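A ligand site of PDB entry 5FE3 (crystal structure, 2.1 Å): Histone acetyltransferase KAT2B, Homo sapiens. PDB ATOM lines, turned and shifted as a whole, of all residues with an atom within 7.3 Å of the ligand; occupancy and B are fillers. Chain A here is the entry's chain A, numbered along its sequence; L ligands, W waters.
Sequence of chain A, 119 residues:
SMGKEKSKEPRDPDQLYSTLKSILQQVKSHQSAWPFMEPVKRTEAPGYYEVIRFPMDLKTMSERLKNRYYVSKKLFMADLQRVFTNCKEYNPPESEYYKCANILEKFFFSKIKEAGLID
Water W1 lies within hydrogen-bond range of the side-chain hydroxyl of Tyr 48 (2.7 Å), a nitrogen (N2) of the ligand (2.9 Å) and the backbone NH of Cys 87 (3.3 Å). Water W2 lies within hydrogen-bond range of O of Pro 35 (2.8 Å), O of Glu 38 (2.9 Å) and N1 of the ligand (3.4 Å).
CD1 of Phe 36 touches N1 of the ligand, 3.9 Å away. Val 40 touches the ligand. Glu 44 touches the ligand. Ala 45 touches the ligand (CB to C6, 3.9 Å). Tyr 97 touches the ligand. Hydrophobic or aromatic side chains within 4 Å of the ligand: Pro 35, Phe 36, Val 40, Ala 45 and Tyr 97. Seven residues have an atom within 4 Å of the ligand: Pro 35, Phe 36, Val 40, Glu 44, Ala 45, Asn 91 and Tyr 97. Along chain A the residues within 4 Å of the ligand span positions 35 to 97. The nearest printed residue that does not touch the ligand is Tyr 48 (4.04 Å).
The backbone carbonyl oxygen of Cys 87 lies within hydrogen-bond range of the side-chain amide nitrogen of Asn 91, at 3.0 Å. The backbone carbonyl oxygen of Tyr 97 sits at hydrogen-bond distance from the side-chain sulfur of Cys 87, at 3.3 Å.
A nitrogen (N1) of the ligand lies within hydrogen-bond range of the backbone carbonyl oxygen (O) of Pro 35 (2.9 Å). The side-chain amide nitrogen of Asn 91 sits at hydrogen-bond distance from an oxygen (O2) of the ligand.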
ATOM      1  N   TRP A  34     -27.756  33.378  -6.431  1.00  0.00           N
ATOM      2  CA  TRP A  34     -28.541  32.479  -5.529  1.00  0.00           C
ATOM      3  C   TRP A  34     -28.858  31.121  -6.143  1.00  0.00           C
ATOM      4  O   TRP A  34     -28.810  30.146  -5.433  1.00  0.00           O
ATOM      5  CB  TRP A  34     -29.802  33.170  -4.976  1.00  0.00           C
ATOM      6  CG  TRP A  34     -30.767  33.657  -6.007  1.00  0.00           C
ATOM      7  CD1 TRP A  34     -30.791  34.910  -6.588  1.00  0.00           C
ATOM      8  CD2 TRP A  34     -31.814  32.913  -6.617  1.00  0.00           C
ATOM      9  NE1 TRP A  34     -31.792  34.981  -7.515  1.00  0.00           N
ATOM     10  CE2 TRP A  34     -32.429  33.771  -7.568  1.00  0.00           C
ATOM     11  CE3 TRP A  34     -32.254  31.593  -6.507  1.00  0.00           C
ATOM     12  CZ2 TRP A  34     -33.505  33.362  -8.358  1.00  0.00           C
ATOM     13  CZ3 TRP A  34     -33.311  31.188  -7.264  1.00  0.00           C
ATOM     14  CH2 TRP A  34     -33.923  32.062  -8.190  1.00  0.00           C
ATOM     15  N   PRO A  35     -29.101  31.038  -7.468  1.00  0.00           N
ATOM     16  CA  PRO A  35     -29.381  29.717  -8.048  1.00  0.00           C
ATOM     17  C   PRO A  35     -28.212  28.740  -8.052  1.00  0.00           C
ATOM     18  O   PRO A  35     -28.437  27.541  -8.202  1.00  0.00           O
ATOM     19  CB  PRO A  35     -29.739  30.049  -9.525  1.00  0.00           C
ATOM     20  CG  PRO A  35     -30.173  31.467  -9.503  1.00  0.00           C
ATOM     21  CD  PRO A  35     -29.209  32.079  -8.514  1.00  0.00           C
ATOM     22  N   PHE A  36     -26.997  29.262  -7.883  1.00  0.00           N
ATOM     23  CA  PHE A  36     -25.782  28.510  -8.047  1.00  0.00           C
ATOM     24  C   PHE A  36     -25.045  28.193  -6.752  1.00  0.00           C
ATOM     25  O   PHE A  36     -23.904  27.733  -6.789  1.00  0.00           O
ATOM     26  CB  PHE A  36     -24.848  29.270  -9.037  1.00  0.00           C
ATOM     27  CG  PHE A  36     -25.595  29.787 -10.259  1.00  0.00           C
ATOM     28  CD1 PHE A  36     -26.148  28.904 -11.139  1.00  0.00           C
ATOM     29  CD2 PHE A  36     -25.890  31.129 -10.401  1.00  0.00           C
ATOM     30  CE1 PHE A  36     -26.929  29.333 -12.193  1.00  0.00           C
ATOM     31  CE2 PHE A  36     -26.630  31.592 -11.480  1.00  0.00           C
ATOM     32  CZ  PHE A  36     -27.165  30.699 -12.366  1.00  0.00           C
ATOM     33  N   MET A  37     -25.672  28.498  -5.626  1.00  0.00           N
ATOM     34  CA  MET A  37     -24.998  28.428  -4.342  1.00  0.00           C
ATOM     35  C   MET A  37     -24.736  27.028  -3.838  1.00  0.00           C
ATOM     36  O   MET A  37     -23.769  26.858  -3.167  1.00  0.00           O
ATOM     37  CB  MET A  37     -25.727  29.240  -3.262  1.00  0.00           C
ATOM     38  CG  MET A  37     -25.684  30.749  -3.524  1.00  0.00           C
ATOM     39  SD  MET A  37     -23.991  31.384  -3.440  1.00  0.00           S
ATOM     40  CE  MET A  37     -23.760  31.311  -1.668  1.00  0.00           C
ATOM     41  N   GLU A  38     -25.509  26.028  -4.267  1.00  0.00           N
ATOM     42  CA  GLU A  38     -25.330  24.627  -3.876  1.00  0.00           C
ATOM     43  C   GLU A  38     -25.606  23.685  -5.036  1.00  0.00           C
ATOM     44  O   GLU A  38     -26.263  24.074  -5.967  1.00  0.00           O
ATOM     45  CB  GLU A  38     -26.321  24.277  -2.741  1.00  0.00           C
ATOM     46  CG  GLU A  38     -26.061  25.059  -1.476  1.00  0.00           C
ATOM     47  CD  GLU A  38     -26.887  24.595  -0.292  1.00  0.00           C
ATOM     48  OE1 GLU A  38     -27.909  23.890  -0.464  1.00  0.00           O
ATOM     49  OE2 GLU A  38     -26.508  24.965   0.837  1.00  0.00           O
ATOM     50  N   PRO A  39     -25.168  22.404  -4.944  1.00  0.00           N
ATOM     51  CA  PRO A  39     -25.500  21.437  -6.000  1.00  0.00           C
ATOM     52  C   PRO A  39     -26.989  21.353  -6.337  1.00  0.00           C
ATOM     53  O   PRO A  39     -27.851  21.376  -5.441  1.00  0.00           O
ATOM     54  CB  PRO A  39     -25.018  20.080  -5.409  1.00  0.00           C
ATOM     55  CG  PRO A  39     -23.898  20.448  -4.513  1.00  0.00           C
ATOM     56  CD  PRO A  39     -24.311  21.774  -3.897  1.00  0.00           C
ATOM     57  N   VAL A  40     -27.276  21.266  -7.631  1.00  0.00           N
ATOM     58  CA  VAL A  40     -28.634  20.996  -8.096  1.00  0.00           C
ATOM     59  C   VAL A  40     -29.105  19.670  -7.490  1.00  0.00           C
ATOM     60  O   VAL A  40     -28.356  18.709  -7.485  1.00  0.00           O
ATOM     61  CB  VAL A  40     -28.680  20.921  -9.655  1.00  0.00           C
ATOM     62  CG1 VAL A  40     -30.074  20.494 -10.147  1.00  0.00           C
ATOM     63  CG2 VAL A  40     -28.341  22.264 -10.238  1.00  0.00           C
ATOM     64  N   LYS A  41     -30.334  19.626  -6.966  1.00  0.00           N
ATOM     65  CA  LYS A  41     -30.883  18.375  -6.450  1.00  0.00           C
ATOM     66  C   LYS A  41     -31.619  17.601  -7.542  1.00  0.00           C
ATOM     67  O   LYS A  41     -32.389  18.182  -8.290  1.00  0.00           O
ATOM     68  CB  LYS A  41     -31.889  18.637  -5.352  1.00  0.00           C
ATOM     69  CG  LYS A  41     -31.357  19.366  -4.156  1.00  0.00           C
ATOM     70  CD  LYS A  41     -32.367  19.198  -3.018  1.00  0.00           C
ATOM     71  CE  LYS A  41     -32.491  20.434  -2.150  1.00  0.00           C
ATOM     72  NZ  LYS A  41     -31.153  20.935  -1.774  1.00  0.00           N
ATOM     73  N   GLU A  44     -35.358  18.152  -7.513  1.00  0.00           N
ATOM     74  CA  GLU A  44     -35.838  19.399  -8.081  1.00  0.00           C
ATOM     75  C   GLU A  44     -35.543  19.526  -9.558  1.00  0.00           C
ATOM     76  O   GLU A  44     -35.958  20.506 -10.184  1.00  0.00           O
ATOM     77  CB  GLU A  44     -35.249  20.595  -7.347  1.00  0.00           C
ATOM     78  CG  GLU A  44     -35.584  20.603  -5.872  1.00  0.00           C
ATOM     79  CD  GLU A  44     -34.993  21.773  -5.121  1.00  0.00           C
ATOM     80  OE1 GLU A  44     -34.211  22.556  -5.697  1.00  0.00           O
ATOM     81  OE2 GLU A  44     -35.386  21.945  -3.962  1.00  0.00           O
ATOM     82  N   ALA A  45     -34.774  18.614 -10.158  1.00  0.00           N
ATOM     83  CA  ALA A  45     -34.533  18.799 -11.572  1.00  0.00           C
ATOM     84  C   ALA A  45     -34.593  17.541 -12.389  1.00  0.00           C
ATOM     85  O   ALA A  45     -33.551  16.937 -12.648  1.00  0.00           O
ATOM     86  CB  ALA A  45     -33.232  19.544 -11.793  1.00  0.00           C
ATOM     87  N   PRO A  46     -35.803  17.161 -12.841  1.00  0.00           N
ATOM     88  CA  PRO A  46     -35.943  15.871 -13.536  1.00  0.00           C
ATOM     89  C   PRO A  46     -34.996  15.790 -14.759  1.00  0.00           C
ATOM     90  O   PRO A  46     -34.914  16.725 -15.548  1.00  0.00           O
ATOM     91  CB  PRO A  46     -37.433  15.832 -13.973  1.00  0.00           C
ATOM     92  CG  PRO A  46     -38.111  16.893 -13.165  1.00  0.00           C
ATOM     93  CD  PRO A  46     -37.079  17.913 -12.815  1.00  0.00           C
ATOM     94  N   TYR A  48     -31.854  16.141 -14.944  1.00  0.00           N
ATOM     95  CA  TYR A  48     -30.671  16.967 -14.873  1.00  0.00           C
ATOM     96  C   TYR A  48     -29.387  16.155 -15.040  1.00  0.00           C
ATOM     97  O   TYR A  48     -28.600  16.419 -15.949  1.00  0.00           O
ATOM     98  CB  TYR A  48     -30.603  17.736 -13.562  1.00  0.00           C
ATOM     99  CG  TYR A  48     -29.536  18.787 -13.557  1.00  0.00           C
ATOM    100  CD1 TYR A  48     -28.237  18.504 -13.113  1.00  0.00           C
ATOM    101  CD2 TYR A  48     -29.798  20.075 -14.025  1.00  0.00           C
ATOM    102  CE1 TYR A  48     -27.241  19.470 -13.119  1.00  0.00           C
ATOM    103  CE2 TYR A  48     -28.810  21.054 -14.015  1.00  0.00           C
ATOM    104  CZ  TYR A  48     -27.538  20.746 -13.564  1.00  0.00           C
ATOM    105  OH  TYR A  48     -26.559  21.690 -13.555  1.00  0.00           O
ATOM    106  N   MET A  56     -21.585  21.589 -11.459  1.00  0.00           N
ATOM    107  CA  MET A  56     -20.706  22.462 -10.693  1.00  0.00           C
ATOM    108  C   MET A  56     -21.570  23.518 -10.011  1.00  0.00           C
ATOM    109  O   MET A  56     -22.612  23.901 -10.528  1.00  0.00           O
ATOM    110  CB  MET A  56     -19.625  23.080 -11.626  1.00  0.00           C
ATOM    111  CG  MET A  56     -18.518  23.848 -10.916  1.00  0.00           C
ATOM    112  SD  MET A  56     -17.805  23.031  -9.415  1.00  0.00           S
ATOM    113  CE  MET A  56     -17.200  21.484 -10.129  1.00  0.00           C
ATOM    114  N   VAL A  83     -20.605  26.329 -14.477  1.00  0.00           N
ATOM    115  CA  VAL A  83     -21.823  26.673 -13.703  1.00  0.00           C
ATOM    116  C   VAL A  83     -22.839  27.370 -14.627  1.00  0.00           C
ATOM    117  O   VAL A  83     -24.026  27.012 -14.666  1.00  0.00           O
ATOM    118  CB  VAL A  83     -21.468  27.641 -12.542  1.00  0.00           C
ATOM    119  CG1 VAL A  83     -22.747  28.170 -11.870  1.00  0.00           C
ATOM    120  CG2 VAL A  83     -20.573  26.944 -11.524  1.00  0.00           C
ATOM    121  N   ASN A  86     -23.942  24.924 -17.808  1.00  0.00           N
ATOM    122  CA  ASN A  86     -24.861  23.867 -17.367  1.00  0.00           C
ATOM    123  C   ASN A  86     -26.265  24.423 -17.228  1.00  0.00           C
ATOM    124  O   ASN A  86     -27.265  23.863 -17.747  1.00  0.00           O
ATOM    125  CB  ASN A  86     -24.412  23.265 -16.032  1.00  0.00           C
ATOM    126  CG  ASN A  86     -23.178  22.393 -16.145  1.00  0.00           C
ATOM    127  OD1 ASN A  86     -22.768  22.011 -17.240  1.00  0.00           O
ATOM    128  ND2 ASN A  86     -22.584  22.076 -15.005  1.00  0.00           N
ATOM    129  N   CYS A  87     -26.346  25.555 -16.570  1.00  0.00           N
ATOM    130  CA  CYS A  87     -27.630  26.217 -16.331  1.00  0.00           C
ATOM    131  C   CYS A  87     -28.334  26.538 -17.643  1.00  0.00           C
ATOM    132  O   CYS A  87     -29.520  26.268 -17.810  1.00  0.00           O
ATOM    133  CB  CYS A  87     -27.407  27.468 -15.510  1.00  0.00           C
ATOM    134  SG  CYS A  87     -28.918  28.406 -15.217  1.00  0.00           S
ATOM    135  N   LYS A  88     -27.595  27.107 -18.579  1.00  0.00           N
ATOM    136  CA  LYS A  88     -28.173  27.542 -19.831  1.00  0.00           C
ATOM    137  C   LYS A  88     -28.584  26.385 -20.724  1.00  0.00           C
ATOM    138  O   LYS A  88     -29.519  26.533 -21.489  1.00  0.00           O
ATOM    139  CB  LYS A  88     -27.225  28.494 -20.565  1.00  0.00           C
ATOM    140  CG  LYS A  88     -27.164  29.840 -19.877  1.00  0.00           C
ATOM    141  CD  LYS A  88     -26.390  30.894 -20.699  1.00  0.00           C
ATOM    142  CE  LYS A  88     -24.980  30.987 -20.255  1.00  0.00           C
ATOM    143  NZ  LYS A  88     -24.227  31.947 -21.099  1.00  0.00           N
ATOM    144  N   TYR A  90     -29.789  23.496 -19.518  1.00  0.00           N
ATOM    145  CA  TYR A  90     -30.877  22.793 -18.864  1.00  0.00           C
ATOM    146  C   TYR A  90     -32.178  23.611 -18.843  1.00  0.00           C
ATOM    147  O   TYR A  90     -33.260  23.074 -19.048  1.00  0.00           O
ATOM    148  CB  TYR A  90     -30.494  22.422 -17.435  1.00  0.00           C
ATOM    149  CG  TYR A  90     -31.565  21.580 -16.776  1.00  0.00           C
ATOM    150  CD1 TYR A  90     -31.785  20.262 -17.196  1.00  0.00           C
ATOM    151  CD2 TYR A  90     -32.406  22.104 -15.788  1.00  0.00           C
ATOM    152  CE1 TYR A  90     -32.791  19.486 -16.632  1.00  0.00           C
ATOM    153  CE2 TYR A  90     -33.413  21.331 -15.201  1.00  0.00           C
ATOM    154  CZ  TYR A  90     -33.600  20.023 -15.630  1.00  0.00           C
ATOM    155  OH  TYR A  90     -34.593  19.250 -15.093  1.00  0.00           O
ATOM    156  N   ASN A  91     -32.056  24.901 -18.564  1.00  0.00           N
ATOM    157  CA  ASN A  91     -33.223  25.751 -18.324  1.00  0.00           C
ATOM    158  C   ASN A  91     -33.729  26.489 -19.574  1.00  0.00           C
ATOM    159  O   ASN A  91     -32.925  26.787 -20.459  1.00  0.00           O
ATOM    160  CB  ASN A  91     -32.882  26.725 -17.236  1.00  0.00           C
ATOM    161  CG  ASN A  91     -32.640  26.035 -15.901  1.00  0.00           C
ATOM    162  OD1 ASN A  91     -33.574  25.631 -15.249  1.00  0.00           O
ATOM    163  ND2 ASN A  91     -31.397  25.883 -15.526  1.00  0.00           N
ATOM    164  N   TYR A  97     -33.586  31.444 -13.912  1.00  0.00           N
ATOM    165  CA  TYR A  97     -32.266  30.855 -13.749  1.00  0.00           C
ATOM    166  C   TYR A  97     -31.343  31.208 -14.927  1.00  0.00           C
ATOM    167  O   TYR A  97     -30.162  31.470 -14.719  1.00  0.00           O
ATOM    168  CB  TYR A  97     -32.303  29.339 -13.589  1.00  0.00           C
ATOM    169  CG  TYR A  97     -33.085  28.799 -12.406  1.00  0.00           C
ATOM    170  CD1 TYR A  97     -33.002  29.355 -11.149  1.00  0.00           C
ATOM    171  CD2 TYR A  97     -33.891  27.665 -12.568  1.00  0.00           C
ATOM    172  CE1 TYR A  97     -33.725  28.811 -10.076  1.00  0.00           C
ATOM    173  CE2 TYR A  97     -34.613  27.119 -11.517  1.00  0.00           C
ATOM    174  CZ  TYR A  97     -34.525  27.691 -10.271  1.00  0.00           C
ATOM    175  OH  TYR A  97     -35.243  27.094  -9.294  1.00  0.00           O
ATOM    176  N   TYR A  98     -31.893  31.125 -16.146  1.00  0.00           N
ATOM    177  CA  TYR A  98     -31.128  31.452 -17.357  1.00  0.00           C
ATOM    178  C   TYR A  98     -30.746  32.929 -17.314  1.00  0.00           C
ATOM    179  O   TYR A  98     -29.599  33.254 -17.525  1.00  0.00           O
ATOM    180  CB  TYR A  98     -31.909  31.078 -18.632  1.00  0.00           C
ATOM    181  CG  TYR A  98     -31.083  30.953 -19.900  1.00  0.00           C
ATOM    182  CD1 TYR A  98     -30.431  32.064 -20.452  1.00  0.00           C
ATOM    183  CD2 TYR A  98     -30.951  29.734 -20.554  1.00  0.00           C
ATOM    184  CE1 TYR A  98     -29.652  31.948 -21.616  1.00  0.00           C
ATOM    185  CE2 TYR A  98     -30.193  29.612 -21.736  1.00  0.00           C
ATOM    186  CZ  TYR A  98     -29.561  30.736 -22.259  1.00  0.00           C
ATOM    187  OH  TYR A  98     -28.789  30.615 -23.360  1.00  0.00           O
HETATM  188  C1  LIG L   1     -31.954  26.385  -7.684  1.00  0.00           C
HETATM  189  O1  LIG L   1     -31.070  25.753  -8.629  1.00  0.00           O
HETATM  190  C2  LIG L   1     -31.659  24.948  -9.592  1.00  0.00           C
HETATM  191  C3  LIG L   1     -31.075  24.948 -10.817  1.00  0.00           C
HETATM  192  C4  LIG L   1     -30.023  25.587 -11.343  1.00  0.00           C
HETATM  193  N1  LIG L   1     -29.191  26.448 -10.781  1.00  0.00           N
HETATM  194  N2  LIG L   1     -29.871  25.232 -12.604  1.00  0.00           N
HETATM  195  O2  LIG L   1     -30.768  24.407 -12.900  1.00  0.00           O
HETATM  196  C5  LIG L   1     -31.558  24.193 -11.808  1.00  0.00           C
HETATM  197  C6  LIG L   1     -32.646  23.412 -11.640  1.00  0.00           C
HETATM  198  C7  LIG L   1     -33.284  23.367 -10.394  1.00  0.00           C
HETATM  199  C8  LIG L   1     -32.781  24.142  -9.346  1.00  0.00           C
HETATM  200  O   HOH W   1     -27.534  24.141 -13.874  1.00  0.00           O
HETATM  201  O   HOH W   2     -26.985  25.146  -8.515  1.00  0.00           O
